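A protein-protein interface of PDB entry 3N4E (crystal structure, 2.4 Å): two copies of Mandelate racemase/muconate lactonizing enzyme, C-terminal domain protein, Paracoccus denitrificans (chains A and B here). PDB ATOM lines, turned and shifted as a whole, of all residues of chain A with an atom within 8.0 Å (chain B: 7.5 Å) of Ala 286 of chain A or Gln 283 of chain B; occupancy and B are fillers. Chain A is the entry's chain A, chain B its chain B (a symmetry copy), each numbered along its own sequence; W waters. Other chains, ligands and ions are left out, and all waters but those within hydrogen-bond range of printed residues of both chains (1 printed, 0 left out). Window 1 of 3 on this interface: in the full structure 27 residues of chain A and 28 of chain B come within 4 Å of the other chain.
The backbone carbonyl oxygen (O) of His 289 of chain A lies within hydrogen-bond range of the side-chain amide nitrogen (NE2) of Gln 255 of chain B (3.1 Å).
Among the printed residues, pairs that only touch across the chains: Ala 286 of chain A with Leu 254 of chain B (3.5 Å), Ala 290 of chain A with Gln 255 of chain B (3.5 Å), Leu 254 of chain A with Ala 286 of chain B (3.6 Å), Ala 290 of chain A with Leu 254 of chain B (3.6 Å), Ala 290 of chain A with Leu 287 of chain B (3.8 Å), Gln 283 of chain A with Ala 286 of chain B (3.8 Å), Ala 286 of chain A with Gln 283 of chain B (3.9 Å), Leu 287 of chain A with Leu 287 of chain B (3.9 Å) and His 291 of chain A with Leu 287 of chain B (3.9 Å).
Of chain B, only Leu 254 (3.5 Å) and Gln 283 (3.9 Å) come within 4 Å of Ala 286 of chain A. Of the printed residues of chain A, Ala 286 of chain B touches Leu 254 and Gln 283. Printed residues of chain A within 4 Å of Leu 254 of chain B: Ala 286 (3.5 Å) and Ala 290 (3.6 Å). Printed residues of chain B within 4 Å of His 289 of chain A: Gln 255 (3.1 Å). His 289 of chain B touches none of the printed residues of chain A. Val 293 of chain A touches none of the printed residues of chain B.
Of the 21 printed residues of chain A, 7 touch a printed residue of chain B. Hydrophobic or aromatic side chains of chain A that line the printed part of chain B: Leu 254, Ala 286, Leu 287, His 289, Ala 290 and His 291. Of the 21 printed residues of chain B, 5 touch a printed residue of chain A. Printed residues of chain B that touch a printed residue of chain A: Leu 254, Gln 255, Gln 283, Ala 286 and Leu 287. Among the printed residues, 10 pairs touch across the chains. Among the printed residues, no Asp or Glu carboxylate lies within 4 Å of a Lys or Arg side-chain nitrogen of the other chain.
Leu 254 of chain A touches Ala 286 of chain B, and with the chains exchanged Ala 286 of chain A touches Leu 254 of chain B. Gln 283 of chain A touches Ala 286 of chain B, and with the chains exchanged Ala 286 of chain A touches Gln 283 of chain B. Leu 287 of chain B touches its own counterpart, Leu 287 of chain A. 13 positions are printed for both chains. Of the 10 pairs that touch across the chains among the printed residues, 5 have their exchanged pair printed and touching as well.
Water W1 bridges OD2 of Asp 76 of chain B and O of Thr 315 of chain A.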
ATOM      1  N   LEU A 118       5.797 -28.807  23.970  1.00  0.00           N
ATOM      2  CA  LEU A 118       4.404 -28.388  23.991  1.00  0.00           C
ATOM      3  C   LEU A 118       3.467 -29.259  23.159  1.00  0.00           C
ATOM      4  O   LEU A 118       2.286 -28.888  22.971  1.00  0.00           O
ATOM      5  CB  LEU A 118       4.285 -26.937  23.524  1.00  0.00           C
ATOM      6  CG  LEU A 118       4.823 -25.911  24.523  1.00  0.00           C
ATOM      7  CD1 LEU A 118       4.705 -24.490  23.974  1.00  0.00           C
ATOM      8  CD2 LEU A 118       4.112 -26.058  25.889  1.00  0.00           C
ATOM      9  N   LEU A 254      -5.438 -14.336  33.108  1.00  0.00           N
ATOM     10  CA  LEU A 254      -6.315 -15.286  32.447  1.00  0.00           C
ATOM     11  C   LEU A 254      -7.790 -14.924  32.652  1.00  0.00           C
ATOM     12  O   LEU A 254      -8.583 -15.004  31.715  1.00  0.00           O
ATOM     13  CB  LEU A 254      -6.018 -16.696  32.968  1.00  0.00           C
ATOM     14  CG  LEU A 254      -6.754 -17.905  32.374  1.00  0.00           C
ATOM     15  CD1 LEU A 254      -6.423 -18.096  30.882  1.00  0.00           C
ATOM     16  CD2 LEU A 254      -6.396 -19.146  33.174  1.00  0.00           C
ATOM     17  N   LEU A 257      -8.845 -12.008  30.723  1.00  0.00           N
ATOM     18  CA  LEU A 257      -9.039 -12.480  29.353  1.00  0.00           C
ATOM     19  C   LEU A 257     -10.447 -13.065  29.180  1.00  0.00           C
ATOM     20  O   LEU A 257     -11.141 -12.756  28.210  1.00  0.00           O
ATOM     21  CB  LEU A 257      -7.963 -13.492  28.928  1.00  0.00           C
ATOM     22  CG  LEU A 257      -7.784 -13.625  27.405  1.00  0.00           C
ATOM     23  CD1 LEU A 257      -7.162 -12.347  26.760  1.00  0.00           C
ATOM     24  CD2 LEU A 257      -6.958 -14.850  27.051  1.00  0.00           C
ATOM     25  N   ILE A 261     -13.505 -11.697  26.771  1.00  0.00           N
ATOM     26  CA  ILE A 261     -14.280 -12.552  25.870  1.00  0.00           C
ATOM     27  C   ILE A 261     -15.796 -12.477  26.147  1.00  0.00           C
ATOM     28  O   ILE A 261     -16.598 -12.321  25.207  1.00  0.00           O
ATOM     29  CB  ILE A 261     -13.785 -14.017  25.915  1.00  0.00           C
ATOM     30  CG1 ILE A 261     -12.408 -14.132  25.260  1.00  0.00           C
ATOM     31  CG2 ILE A 261     -14.794 -14.967  25.245  1.00  0.00           C
ATOM     32  CD1 ILE A 261     -11.568 -15.291  25.810  1.00  0.00           C
ATOM     33  N   GLY A 280       1.552 -19.363  30.765  1.00  0.00           N
ATOM     34  CA  GLY A 280       0.324 -18.560  30.785  1.00  0.00           C
ATOM     35  C   GLY A 280      -0.336 -18.424  29.424  1.00  0.00           C
ATOM     36  O   GLY A 280      -1.555 -18.530  29.321  1.00  0.00           O
ATOM     37  N   MET A 281       0.464 -18.198  28.381  1.00  0.00           N
ATOM     38  CA  MET A 281      -0.065 -18.067  27.024  1.00  0.00           C
ATOM     39  C   MET A 281      -0.743 -19.329  26.516  1.00  0.00           C
ATOM     40  O   MET A 281      -1.755 -19.245  25.819  1.00  0.00           O
ATOM     41  CB  MET A 281       1.011 -17.610  26.045  1.00  0.00           C
ATOM     42  CG  MET A 281       1.404 -16.169  26.239  1.00  0.00           C
ATOM     43  SD  MET A 281      -0.024 -14.880  25.863  1.00  0.00           S
ATOM     44  CE  MET A 281       0.215 -14.826  23.932  1.00  0.00           C
ATOM     45  N   MET A 282      -0.201 -20.495  26.870  1.00  0.00           N
ATOM     46  CA  MET A 282      -0.812 -21.762  26.472  1.00  0.00           C
ATOM     47  C   MET A 282      -2.175 -21.944  27.143  1.00  0.00           C
ATOM     48  O   MET A 282      -3.063 -22.598  26.590  1.00  0.00           O
ATOM     49  CB  MET A 282       0.106 -22.953  26.765  1.00  0.00           C
ATOM     50  CG  MET A 282       1.340 -23.038  25.875  1.00  0.00           C
ATOM     51  SD  MET A 282       0.976 -23.236  23.949  1.00  0.00           S
ATOM     52  CE  MET A 282       0.124 -25.001  23.963  1.00  0.00           C
ATOM     53  N   GLN A 283      -2.337 -21.357  28.328  1.00  0.00           N
ATOM     54  CA  GLN A 283      -3.615 -21.378  29.027  1.00  0.00           C
ATOM     55  C   GLN A 283      -4.579 -20.400  28.357  1.00  0.00           C
ATOM     56  O   GLN A 283      -5.768 -20.686  28.209  1.00  0.00           O
ATOM     57  CB  GLN A 283      -3.439 -21.035  30.507  1.00  0.00           C
ATOM     58  CG  GLN A 283      -2.731 -22.101  31.334  1.00  0.00           C
ATOM     59  CD  GLN A 283      -2.508 -21.672  32.786  1.00  0.00           C
ATOM     60  OE1 GLN A 283      -2.661 -20.488  33.146  1.00  0.00           O
ATOM     61  NE2 GLN A 283      -2.127 -22.628  33.626  1.00  0.00           N
ATOM     62  N   CYS A 284      -4.053 -19.253  27.945  1.00  0.00           N
ATOM     63  CA  CYS A 284      -4.824 -18.284  27.185  1.00  0.00           C
ATOM     64  C   CYS A 284      -5.329 -18.874  25.868  1.00  0.00           C
ATOM     65  O   CYS A 284      -6.516 -18.710  25.521  1.00  0.00           O
ATOM     66  CB  CYS A 284      -4.012 -17.007  26.954  1.00  0.00           C
ATOM     67  SG  CYS A 284      -3.785 -16.053  28.490  1.00  0.00           S
ATOM     68  N   ALA A 285      -4.431 -19.571  25.166  1.00  0.00           N
ATOM     69  CA  ALA A 285      -4.759 -20.247  23.915  1.00  0.00           C
ATOM     70  C   ALA A 285      -5.891 -21.242  24.120  1.00  0.00           C
ATOM     71  O   ALA A 285      -6.819 -21.297  23.325  1.00  0.00           O
ATOM     72  CB  ALA A 285      -3.529 -20.940  23.340  1.00  0.00           C
ATOM     73  N   ALA A 286      -5.819 -21.997  25.212  1.00  0.00           N
ATOM     74  CA  ALA A 286      -6.861 -22.953  25.578  1.00  0.00           C
ATOM     75  C   ALA A 286      -8.194 -22.272  25.865  1.00  0.00           C
ATOM     76  O   ALA A 286      -9.216 -22.698  25.350  1.00  0.00           O
ATOM     77  CB  ALA A 286      -6.418 -23.830  26.770  1.00  0.00           C
ATOM     78  N   LEU A 287      -8.188 -21.207  26.666  1.00  0.00           N
ATOM     79  CA  LEU A 287      -9.415 -20.407  26.880  1.00  0.00           C
ATOM     80  C   LEU A 287      -9.976 -19.857  25.558  1.00  0.00           C
ATOM     81  O   LEU A 287     -11.187 -19.830  25.365  1.00  0.00           O
ATOM     82  CB  LEU A 287      -9.167 -19.259  27.864  1.00  0.00           C
ATOM     83  CG  LEU A 287     -10.277 -18.258  28.235  1.00  0.00           C
ATOM     84  CD1 LEU A 287     -11.349 -18.894  29.093  1.00  0.00           C
ATOM     85  CD2 LEU A 287      -9.716 -17.037  28.953  1.00  0.00           C
ATOM     86  N   ALA A 288      -9.101 -19.428  24.653  1.00  0.00           N
ATOM     87  CA  ALA A 288      -9.549 -18.936  23.361  1.00  0.00           C
ATOM     88  C   ALA A 288     -10.258 -20.061  22.604  1.00  0.00           C
ATOM     89  O   ALA A 288     -11.352 -19.881  22.053  1.00  0.00           O
ATOM     90  CB  ALA A 288      -8.374 -18.383  22.558  1.00  0.00           C
ATOM     91  N   HIS A 289      -9.649 -21.238  22.624  1.00  0.00           N
ATOM     92  CA  HIS A 289     -10.218 -22.390  21.955  1.00  0.00           C
ATOM     93  C   HIS A 289     -11.522 -22.888  22.614  1.00  0.00           C
ATOM     94  O   HIS A 289     -12.424 -23.342  21.916  1.00  0.00           O
ATOM     95  CB  HIS A 289      -9.169 -23.496  21.836  1.00  0.00           C
ATOM     96  CG  HIS A 289      -9.604 -24.642  20.986  1.00  0.00           C
ATOM     97  ND1 HIS A 289     -10.065 -24.479  19.695  1.00  0.00           N
ATOM     98  CD2 HIS A 289      -9.664 -25.971  21.246  1.00  0.00           C
ATOM     99  CE1 HIS A 289     -10.394 -25.659  19.198  1.00  0.00           C
ATOM    100  NE2 HIS A 289     -10.166 -26.580  20.119  1.00  0.00           N
ATOM    101  N   ALA A 290     -11.635 -22.772  23.941  1.00  0.00           N
ATOM    102  CA  ALA A 290     -12.889 -23.102  24.628  1.00  0.00           C
ATOM    103  C   ALA A 290     -14.061 -22.196  24.206  1.00  0.00           C
ATOM    104  O   ALA A 290     -15.197 -22.672  24.056  1.00  0.00           O
ATOM    105  CB  ALA A 290     -12.708 -23.079  26.132  1.00  0.00           C
ATOM    106  N   HIS A 291     -13.784 -20.904  24.007  1.00  0.00           N
ATOM    107  CA  HIS A 291     -14.844 -19.933  23.689  1.00  0.00           C
ATOM    108  C   HIS A 291     -15.015 -19.626  22.198  1.00  0.00           C
ATOM    109  O   HIS A 291     -15.865 -18.835  21.827  1.00  0.00           O
ATOM    110  CB  HIS A 291     -14.613 -18.632  24.454  1.00  0.00           C
ATOM    111  CG  HIS A 291     -14.846 -18.760  25.923  1.00  0.00           C
ATOM    112  ND1 HIS A 291     -16.044 -18.431  26.517  1.00  0.00           N
ATOM    113  CD2 HIS A 291     -14.044 -19.215  26.912  1.00  0.00           C
ATOM    114  CE1 HIS A 291     -15.962 -18.658  27.813  1.00  0.00           C
ATOM    115  NE2 HIS A 291     -14.762 -19.136  28.079  1.00  0.00           N
ATOM    116  N   GLY A 292     -14.194 -20.236  21.355  1.00  0.00           N
ATOM    117  CA  GLY A 292     -14.300 -20.051  19.922  1.00  0.00           C
ATOM    118  C   GLY A 292     -13.863 -18.686  19.452  1.00  0.00           C
ATOM    119  O   GLY A 292     -14.395 -18.176  18.486  1.00  0.00           O
ATOM    120  N   VAL A 293     -12.888 -18.086  20.125  1.00  0.00           N
ATOM    121  CA  VAL A 293     -12.395 -16.796  19.693  1.00  0.00           C
ATOM    122  C   VAL A 293     -11.009 -16.932  19.052  1.00  0.00           C
ATOM    123  O   VAL A 293     -10.268 -17.861  19.370  1.00  0.00           O
ATOM    124  CB  VAL A 293     -12.393 -15.753  20.843  1.00  0.00           C
ATOM    125  CG1 VAL A 293     -13.773 -15.704  21.551  1.00  0.00           C
ATOM    126  CG2 VAL A 293     -11.288 -16.028  21.838  1.00  0.00           C
ATOM    127  N   PHE A 295      -7.119 -16.215  18.422  1.00  0.00           N
ATOM    128  CA  PHE A 295      -6.000 -15.990  19.314  1.00  0.00           C
ATOM    129  C   PHE A 295      -4.873 -15.433  18.452  1.00  0.00           C
ATOM    130  O   PHE A 295      -4.363 -16.124  17.569  1.00  0.00           O
ATOM    131  CB  PHE A 295      -5.625 -17.307  19.982  1.00  0.00           C
ATOM    132  CG  PHE A 295      -4.593 -17.177  21.062  1.00  0.00           C
ATOM    133  CD1 PHE A 295      -4.922 -16.645  22.305  1.00  0.00           C
ATOM    134  CD2 PHE A 295      -3.298 -17.622  20.852  1.00  0.00           C
ATOM    135  CE1 PHE A 295      -3.975 -16.533  23.307  1.00  0.00           C
ATOM    136  CE2 PHE A 295      -2.346 -17.516  21.856  1.00  0.00           C
ATOM    137  CZ  PHE A 295      -2.691 -16.968  23.086  1.00  0.00           C
ATOM    138  N   THR A 315       2.048 -24.051  17.801  1.00  0.00           N
ATOM    139  CA  THR A 315       1.196 -25.108  18.380  1.00  0.00           C
ATOM    140  C   THR A 315      -0.294 -24.790  18.289  1.00  0.00           C
ATOM    141  O   THR A 315      -1.131 -25.588  18.740  1.00  0.00           O
ATOM    142  CB  THR A 315       1.484 -25.346  19.884  1.00  0.00           C
ATOM    143  OG1 THR A 315       0.992 -24.234  20.643  1.00  0.00           O
ATOM    144  CG2 THR A 315       2.956 -25.508  20.146  1.00  0.00           C
ATOM    145  N   LEU A 316      -0.620 -23.630  17.721  1.00  0.00           N
ATOM    146  CA  LEU A 316      -1.994 -23.177  17.659  1.00  0.00           C
ATOM    147  C   LEU A 316      -2.659 -23.751  16.419  1.00  0.00           C
ATOM    148  O   LEU A 316      -2.310 -23.412  15.299  1.00  0.00           O
ATOM    149  CB  LEU A 316      -2.053 -21.638  17.664  1.00  0.00           C
ATOM    150  CG  LEU A 316      -3.402 -20.974  17.368  1.00  0.00           C
ATOM    151  CD1 LEU A 316      -4.332 -21.079  18.559  1.00  0.00           C
ATOM    152  CD2 LEU A 316      -3.229 -19.512  16.972  1.00  0.00           C
ATOM    153  N   ALA B  72       0.333 -33.715  20.639  1.00  0.00           N
ATOM    154  CA  ALA B  72      -0.809 -32.792  20.626  1.00  0.00           C
ATOM    155  C   ALA B  72      -1.341 -32.544  19.213  1.00  0.00           C
ATOM    156  O   ALA B  72      -2.544 -32.619  18.981  1.00  0.00           O
ATOM    157  CB  ALA B  72      -0.470 -31.474  21.298  1.00  0.00           C
ATOM    158  N   ASP B  76      -5.053 -33.951  18.065  1.00  0.00           N
ATOM    159  CA  ASP B  76      -5.992 -32.942  17.572  1.00  0.00           C
ATOM    160  C   ASP B  76      -6.348 -33.141  16.102  1.00  0.00           C
ATOM    161  O   ASP B  76      -7.494 -32.919  15.702  1.00  0.00           O
ATOM    162  CB  ASP B  76      -5.456 -31.523  17.781  1.00  0.00           C
ATOM    163  CG  ASP B  76      -5.481 -31.104  19.235  1.00  0.00           C
ATOM    164  OD1 ASP B  76      -5.888 -31.927  20.103  1.00  0.00           O
ATOM    165  OD2 ASP B  76      -5.086 -29.951  19.506  1.00  0.00           O
ATOM    166  N   LEU B 254     -13.799 -29.624  25.548  1.00  0.00           N
ATOM    167  CA  LEU B 254     -13.498 -28.353  26.171  1.00  0.00           C
ATOM    168  C   LEU B 254     -14.653 -27.363  25.990  1.00  0.00           C
ATOM    169  O   LEU B 254     -15.042 -26.665  26.926  1.00  0.00           O
ATOM    170  CB  LEU B 254     -12.186 -27.797  25.609  1.00  0.00           C
ATOM    171  CG  LEU B 254     -11.591 -26.518  26.208  1.00  0.00           C
ATOM    172  CD1 LEU B 254     -11.088 -26.749  27.621  1.00  0.00           C
ATOM    173  CD2 LEU B 254     -10.460 -25.999  25.332  1.00  0.00           C
ATOM    174  N   GLN B 255     -15.224 -27.312  24.794  1.00  0.00           N
ATOM    175  CA  GLN B 255     -16.310 -26.369  24.531  1.00  0.00           C
ATOM    176  C   GLN B 255     -17.576 -26.749  25.289  1.00  0.00           C
ATOM    177  O   GLN B 255     -18.268 -25.869  25.825  1.00  0.00           O
ATOM    178  CB  GLN B 255     -16.576 -26.230  23.032  1.00  0.00           C
ATOM    179  CG  GLN B 255     -15.369 -25.705  22.227  1.00  0.00           C
ATOM    180  CD  GLN B 255     -14.302 -26.757  22.007  1.00  0.00           C
ATOM    181  OE1 GLN B 255     -14.568 -27.941  22.103  1.00  0.00           O
ATOM    182  NE2 GLN B 255     -13.086 -26.321  21.713  1.00  0.00           N
ATOM    183  N   LEU B 257     -17.612 -28.275  28.071  1.00  0.00           N
ATOM    184  CA  LEU B 257     -17.257 -27.936  29.444  1.00  0.00           C
ATOM    185  C   LEU B 257     -17.469 -26.454  29.719  1.00  0.00           C
ATOM    186  O   LEU B 257     -17.996 -26.062  30.788  1.00  0.00           O
ATOM    187  CB  LEU B 257     -15.814 -28.322  29.765  1.00  0.00           C
ATOM    188  CG  LEU B 257     -15.521 -28.366  31.272  1.00  0.00           C
ATOM    189  CD1 LEU B 257     -16.385 -29.435  31.956  1.00  0.00           C
ATOM    190  CD2 LEU B 257     -14.052 -28.627  31.538  1.00  0.00           C
ATOM    191  N   GLY B 276      -9.766 -36.186  26.472  1.00  0.00           N
ATOM    192  CA  GLY B 276      -8.619 -35.281  26.543  1.00  0.00           C
ATOM    193  C   GLY B 276      -7.286 -35.908  26.892  1.00  0.00           C
ATOM    194  O   GLY B 276      -6.266 -35.522  26.336  1.00  0.00           O
ATOM    195  N   GLY B 277      -7.288 -36.877  27.807  1.00  0.00           N
ATOM    196  CA  GLY B 277      -6.043 -37.416  28.343  1.00  0.00           C
ATOM    197  C   GLY B 277      -5.317 -36.348  29.138  1.00  0.00           C
ATOM    198  O   GLY B 277      -5.944 -35.403  29.610  1.00  0.00           O
ATOM    199  N   ILE B 278      -3.998 -36.459  29.279  1.00  0.00           N
ATOM    200  CA  ILE B 278      -3.268 -35.428  30.029  1.00  0.00           C
ATOM    201  C   ILE B 278      -3.370 -34.037  29.371  1.00  0.00           C
ATOM    202  O   ILE B 278      -3.744 -33.074  30.040  1.00  0.00           O
ATOM    203  CB  ILE B 278      -1.820 -35.839  30.308  1.00  0.00           C
ATOM    204  CG1 ILE B 278      -1.800 -36.917  31.400  1.00  0.00           C
ATOM    205  CG2 ILE B 278      -0.979 -34.619  30.752  1.00  0.00           C
ATOM    206  CD1 ILE B 278      -0.707 -37.907  31.253  1.00  0.00           C
ATOM    207  N   THR B 279      -3.073 -33.936  28.071  1.00  0.00           N
ATOM    208  CA  THR B 279      -3.200 -32.670  27.331  1.00  0.00           C
ATOM    209  C   THR B 279      -4.586 -32.036  27.477  1.00  0.00           C
ATOM    210  O   THR B 279      -4.699 -30.862  27.773  1.00  0.00           O
ATOM    211  CB  THR B 279      -2.880 -32.857  25.823  1.00  0.00           C
ATOM    212  OG1 THR B 279      -1.571 -33.402  25.688  1.00  0.00           O
ATOM    213  CG2 THR B 279      -2.934 -31.543  25.059  1.00  0.00           C
ATOM    214  N   GLY B 280      -5.640 -32.815  27.259  1.00  0.00           N
ATOM    215  CA  GLY B 280      -7.002 -32.278  27.312  1.00  0.00           C
ATOM    216  C   GLY B 280      -7.358 -31.778  28.698  1.00  0.00           C
ATOM    217  O   GLY B 280      -7.908 -30.687  28.849  1.00  0.00           O
ATOM    218  N   MET B 281      -7.023 -32.571  29.711  1.00  0.00           N
ATOM    219  CA  MET B 281      -7.365 -32.248  31.092  1.00  0.00           C
ATOM    220  C   MET B 281      -6.660 -30.997  31.590  1.00  0.00           C
ATOM    221  O   MET B 281      -7.286 -30.184  32.274  1.00  0.00           O
ATOM    222  CB  MET B 281      -7.122 -33.442  32.017  1.00  0.00           C
ATOM    223  CG  MET B 281      -8.115 -34.550  31.792  1.00  0.00           C
ATOM    224  SD  MET B 281      -9.910 -34.091  32.400  1.00  0.00           S
ATOM    225  CE  MET B 281      -9.606 -34.559  34.286  1.00  0.00           C
ATOM    226  N   MET B 282      -5.384 -30.831  31.227  1.00  0.00           N
ATOM    227  CA  MET B 282      -4.658 -29.582  31.505  1.00  0.00           C
ATOM    228  C   MET B 282      -5.377 -28.357  30.914  1.00  0.00           C
ATOM    229  O   MET B 282      -5.450 -27.297  31.549  1.00  0.00           O
ATOM    230  CB  MET B 282      -3.209 -29.646  31.033  1.00  0.00           C
ATOM    231  CG  MET B 282      -2.311 -30.567  31.874  1.00  0.00           C
ATOM    232  SD  MET B 282      -2.308 -30.187  33.830  1.00  0.00           S
ATOM    233  CE  MET B 282      -1.091 -28.637  33.838  1.00  0.00           C
ATOM    234  N   GLN B 283      -5.931 -28.511  29.713  1.00  0.00           N
ATOM    235  CA  GLN B 283      -6.761 -27.467  29.115  1.00  0.00           C
ATOM    236  C   GLN B 283      -8.046 -27.206  29.915  1.00  0.00           C
ATOM    237  O   GLN B 283      -8.438 -26.057  30.121  1.00  0.00           O
ATOM    238  CB  GLN B 283      -7.060 -27.784  27.642  1.00  0.00           C
ATOM    239  CG  GLN B 283      -5.829 -27.638  26.738  1.00  0.00           C
ATOM    240  CD  GLN B 283      -6.076 -28.007  25.276  1.00  0.00           C
ATOM    241  OE1 GLN B 283      -7.163 -28.439  24.884  1.00  0.00           O
ATOM    242  NE2 GLN B 283      -5.041 -27.848  24.461  1.00  0.00           N
ATOM    243  N   CYS B 284      -8.683 -28.269  30.390  1.00  0.00           N
ATOM    244  CA  CYS B 284      -9.884 -28.126  31.202  1.00  0.00           C
ATOM    245  C   CYS B 284      -9.598 -27.408  32.536  1.00  0.00           C
ATOM    246  O   CYS B 284     -10.392 -26.565  32.985  1.00  0.00           O
ATOM    247  CB  CYS B 284     -10.513 -29.493  31.441  1.00  0.00           C
ATOM    248  SG  CYS B 284     -11.152 -30.290  29.946  1.00  0.00           S
ATOM    249  N   ALA B 285      -8.465 -27.737  33.154  1.00  0.00           N
ATOM    250  CA  ALA B 285      -8.056 -27.106  34.401  1.00  0.00           C
ATOM    251  C   ALA B 285      -7.878 -25.596  34.222  1.00  0.00           C
ATOM    252  O   ALA B 285      -8.306 -24.812  35.070  1.00  0.00           O
ATOM    253  CB  ALA B 285      -6.754 -27.768  34.959  1.00  0.00           C
ATOM    254  N   ALA B 286      -7.264 -25.201  33.106  1.00  0.00           N
ATOM    255  CA  ALA B 286      -7.079 -23.793  32.759  1.00  0.00           C
ATOM    256  C   ALA B 286      -8.419 -23.079  32.534  1.00  0.00           C
ATOM    257  O   ALA B 286      -8.608 -21.920  32.952  1.00  0.00           O
ATOM    258  CB  ALA B 286      -6.192 -23.665  31.519  1.00  0.00           C
ATOM    259  N   LEU B 287      -9.350 -23.765  31.890  1.00  0.00           N
ATOM    260  CA  LEU B 287     -10.674 -23.198  31.693  1.00  0.00           C
ATOM    261  C   LEU B 287     -11.374 -23.027  33.042  1.00  0.00           C
ATOM    262  O   LEU B 287     -11.967 -21.990  33.295  1.00  0.00           O
ATOM    263  CB  LEU B 287     -11.517 -24.045  30.725  1.00  0.00           C
ATOM    264  CG  LEU B 287     -12.974 -23.638  30.462  1.00  0.00           C
ATOM    265  CD1 LEU B 287     -13.084 -22.263  29.798  1.00  0.00           C
ATOM    266  CD2 LEU B 287     -13.613 -24.649  29.597  1.00  0.00           C
ATOM    267  N   ALA B 288     -11.262 -24.020  33.922  1.00  0.00           N
ATOM    268  CA  ALA B 288     -11.889 -23.934  35.231  1.00  0.00           C
ATOM    269  C   ALA B 288     -11.348 -22.737  36.011  1.00  0.00           C
ATOM    270  O   ALA B 288     -12.112 -21.967  36.600  1.00  0.00           O
ATOM    271  CB  ALA B 288     -11.687 -25.241  36.014  1.00  0.00           C
ATOM    272  N   HIS B 289     -10.029 -22.583  35.993  1.00  0.00           N
ATOM    273  CA  HIS B 289      -9.332 -21.507  36.696  1.00  0.00           C
ATOM    274  C   HIS B 289      -9.660 -20.155  36.071  1.00  0.00           C
ATOM    275  O   HIS B 289      -9.656 -19.131  36.745  1.00  0.00           O
ATOM    276  CB  HIS B 289      -7.815 -21.768  36.658  1.00  0.00           C
ATOM    277  CG  HIS B 289      -7.002 -20.795  37.453  1.00  0.00           C
ATOM    278  ND1 HIS B 289      -7.186 -20.595  38.806  1.00  0.00           N
ATOM    279  CD2 HIS B 289      -5.981 -19.976  37.087  1.00  0.00           C
ATOM    280  CE1 HIS B 289      -6.327 -19.685  39.236  1.00  0.00           C
ATOM    281  NE2 HIS B 289      -5.582 -19.294  38.215  1.00  0.00           N
ATOM    282  N   PHE B 295     -12.338 -27.772  40.162  1.00  0.00           N
ATOM    283  CA  PHE B 295     -11.989 -28.787  39.196  1.00  0.00           C
ATOM    284  C   PHE B 295     -11.753 -30.066  39.983  1.00  0.00           C
ATOM    285  O   PHE B 295     -10.816 -30.145  40.770  1.00  0.00           O
ATOM    286  CB  PHE B 295     -10.726 -28.361  38.455  1.00  0.00           C
ATOM    287  CG  PHE B 295     -10.357 -29.261  37.311  1.00  0.00           C
ATOM    288  CD1 PHE B 295     -11.095 -29.250  36.134  1.00  0.00           C
ATOM    289  CD2 PHE B 295      -9.248 -30.092  37.402  1.00  0.00           C
ATOM    290  CE1 PHE B 295     -10.757 -30.065  35.067  1.00  0.00           C
ATOM    291  CE2 PHE B 295      -8.887 -30.912  36.335  1.00  0.00           C
ATOM    292  CZ  PHE B 295      -9.656 -30.906  35.162  1.00  0.00           C
ATOM    293  N   VAL B 312      -1.920 -35.021  36.817  1.00  0.00           N
ATOM    294  CA  VAL B 312      -2.634 -33.779  36.546  1.00  0.00           C
ATOM    295  C   VAL B 312      -3.003 -33.029  37.846  1.00  0.00           C
ATOM    296  O   VAL B 312      -2.737 -31.826  37.990  1.00  0.00           O
ATOM    297  CB  VAL B 312      -3.879 -34.020  35.643  1.00  0.00           C
ATOM    298  CG1 VAL B 312      -4.845 -32.838  35.703  1.00  0.00           C
ATOM    299  CG2 VAL B 312      -3.440 -34.298  34.162  1.00  0.00           C
HETATM  300  O   HOH W   1      -3.284 -28.202  18.575  1.00  0.00           O
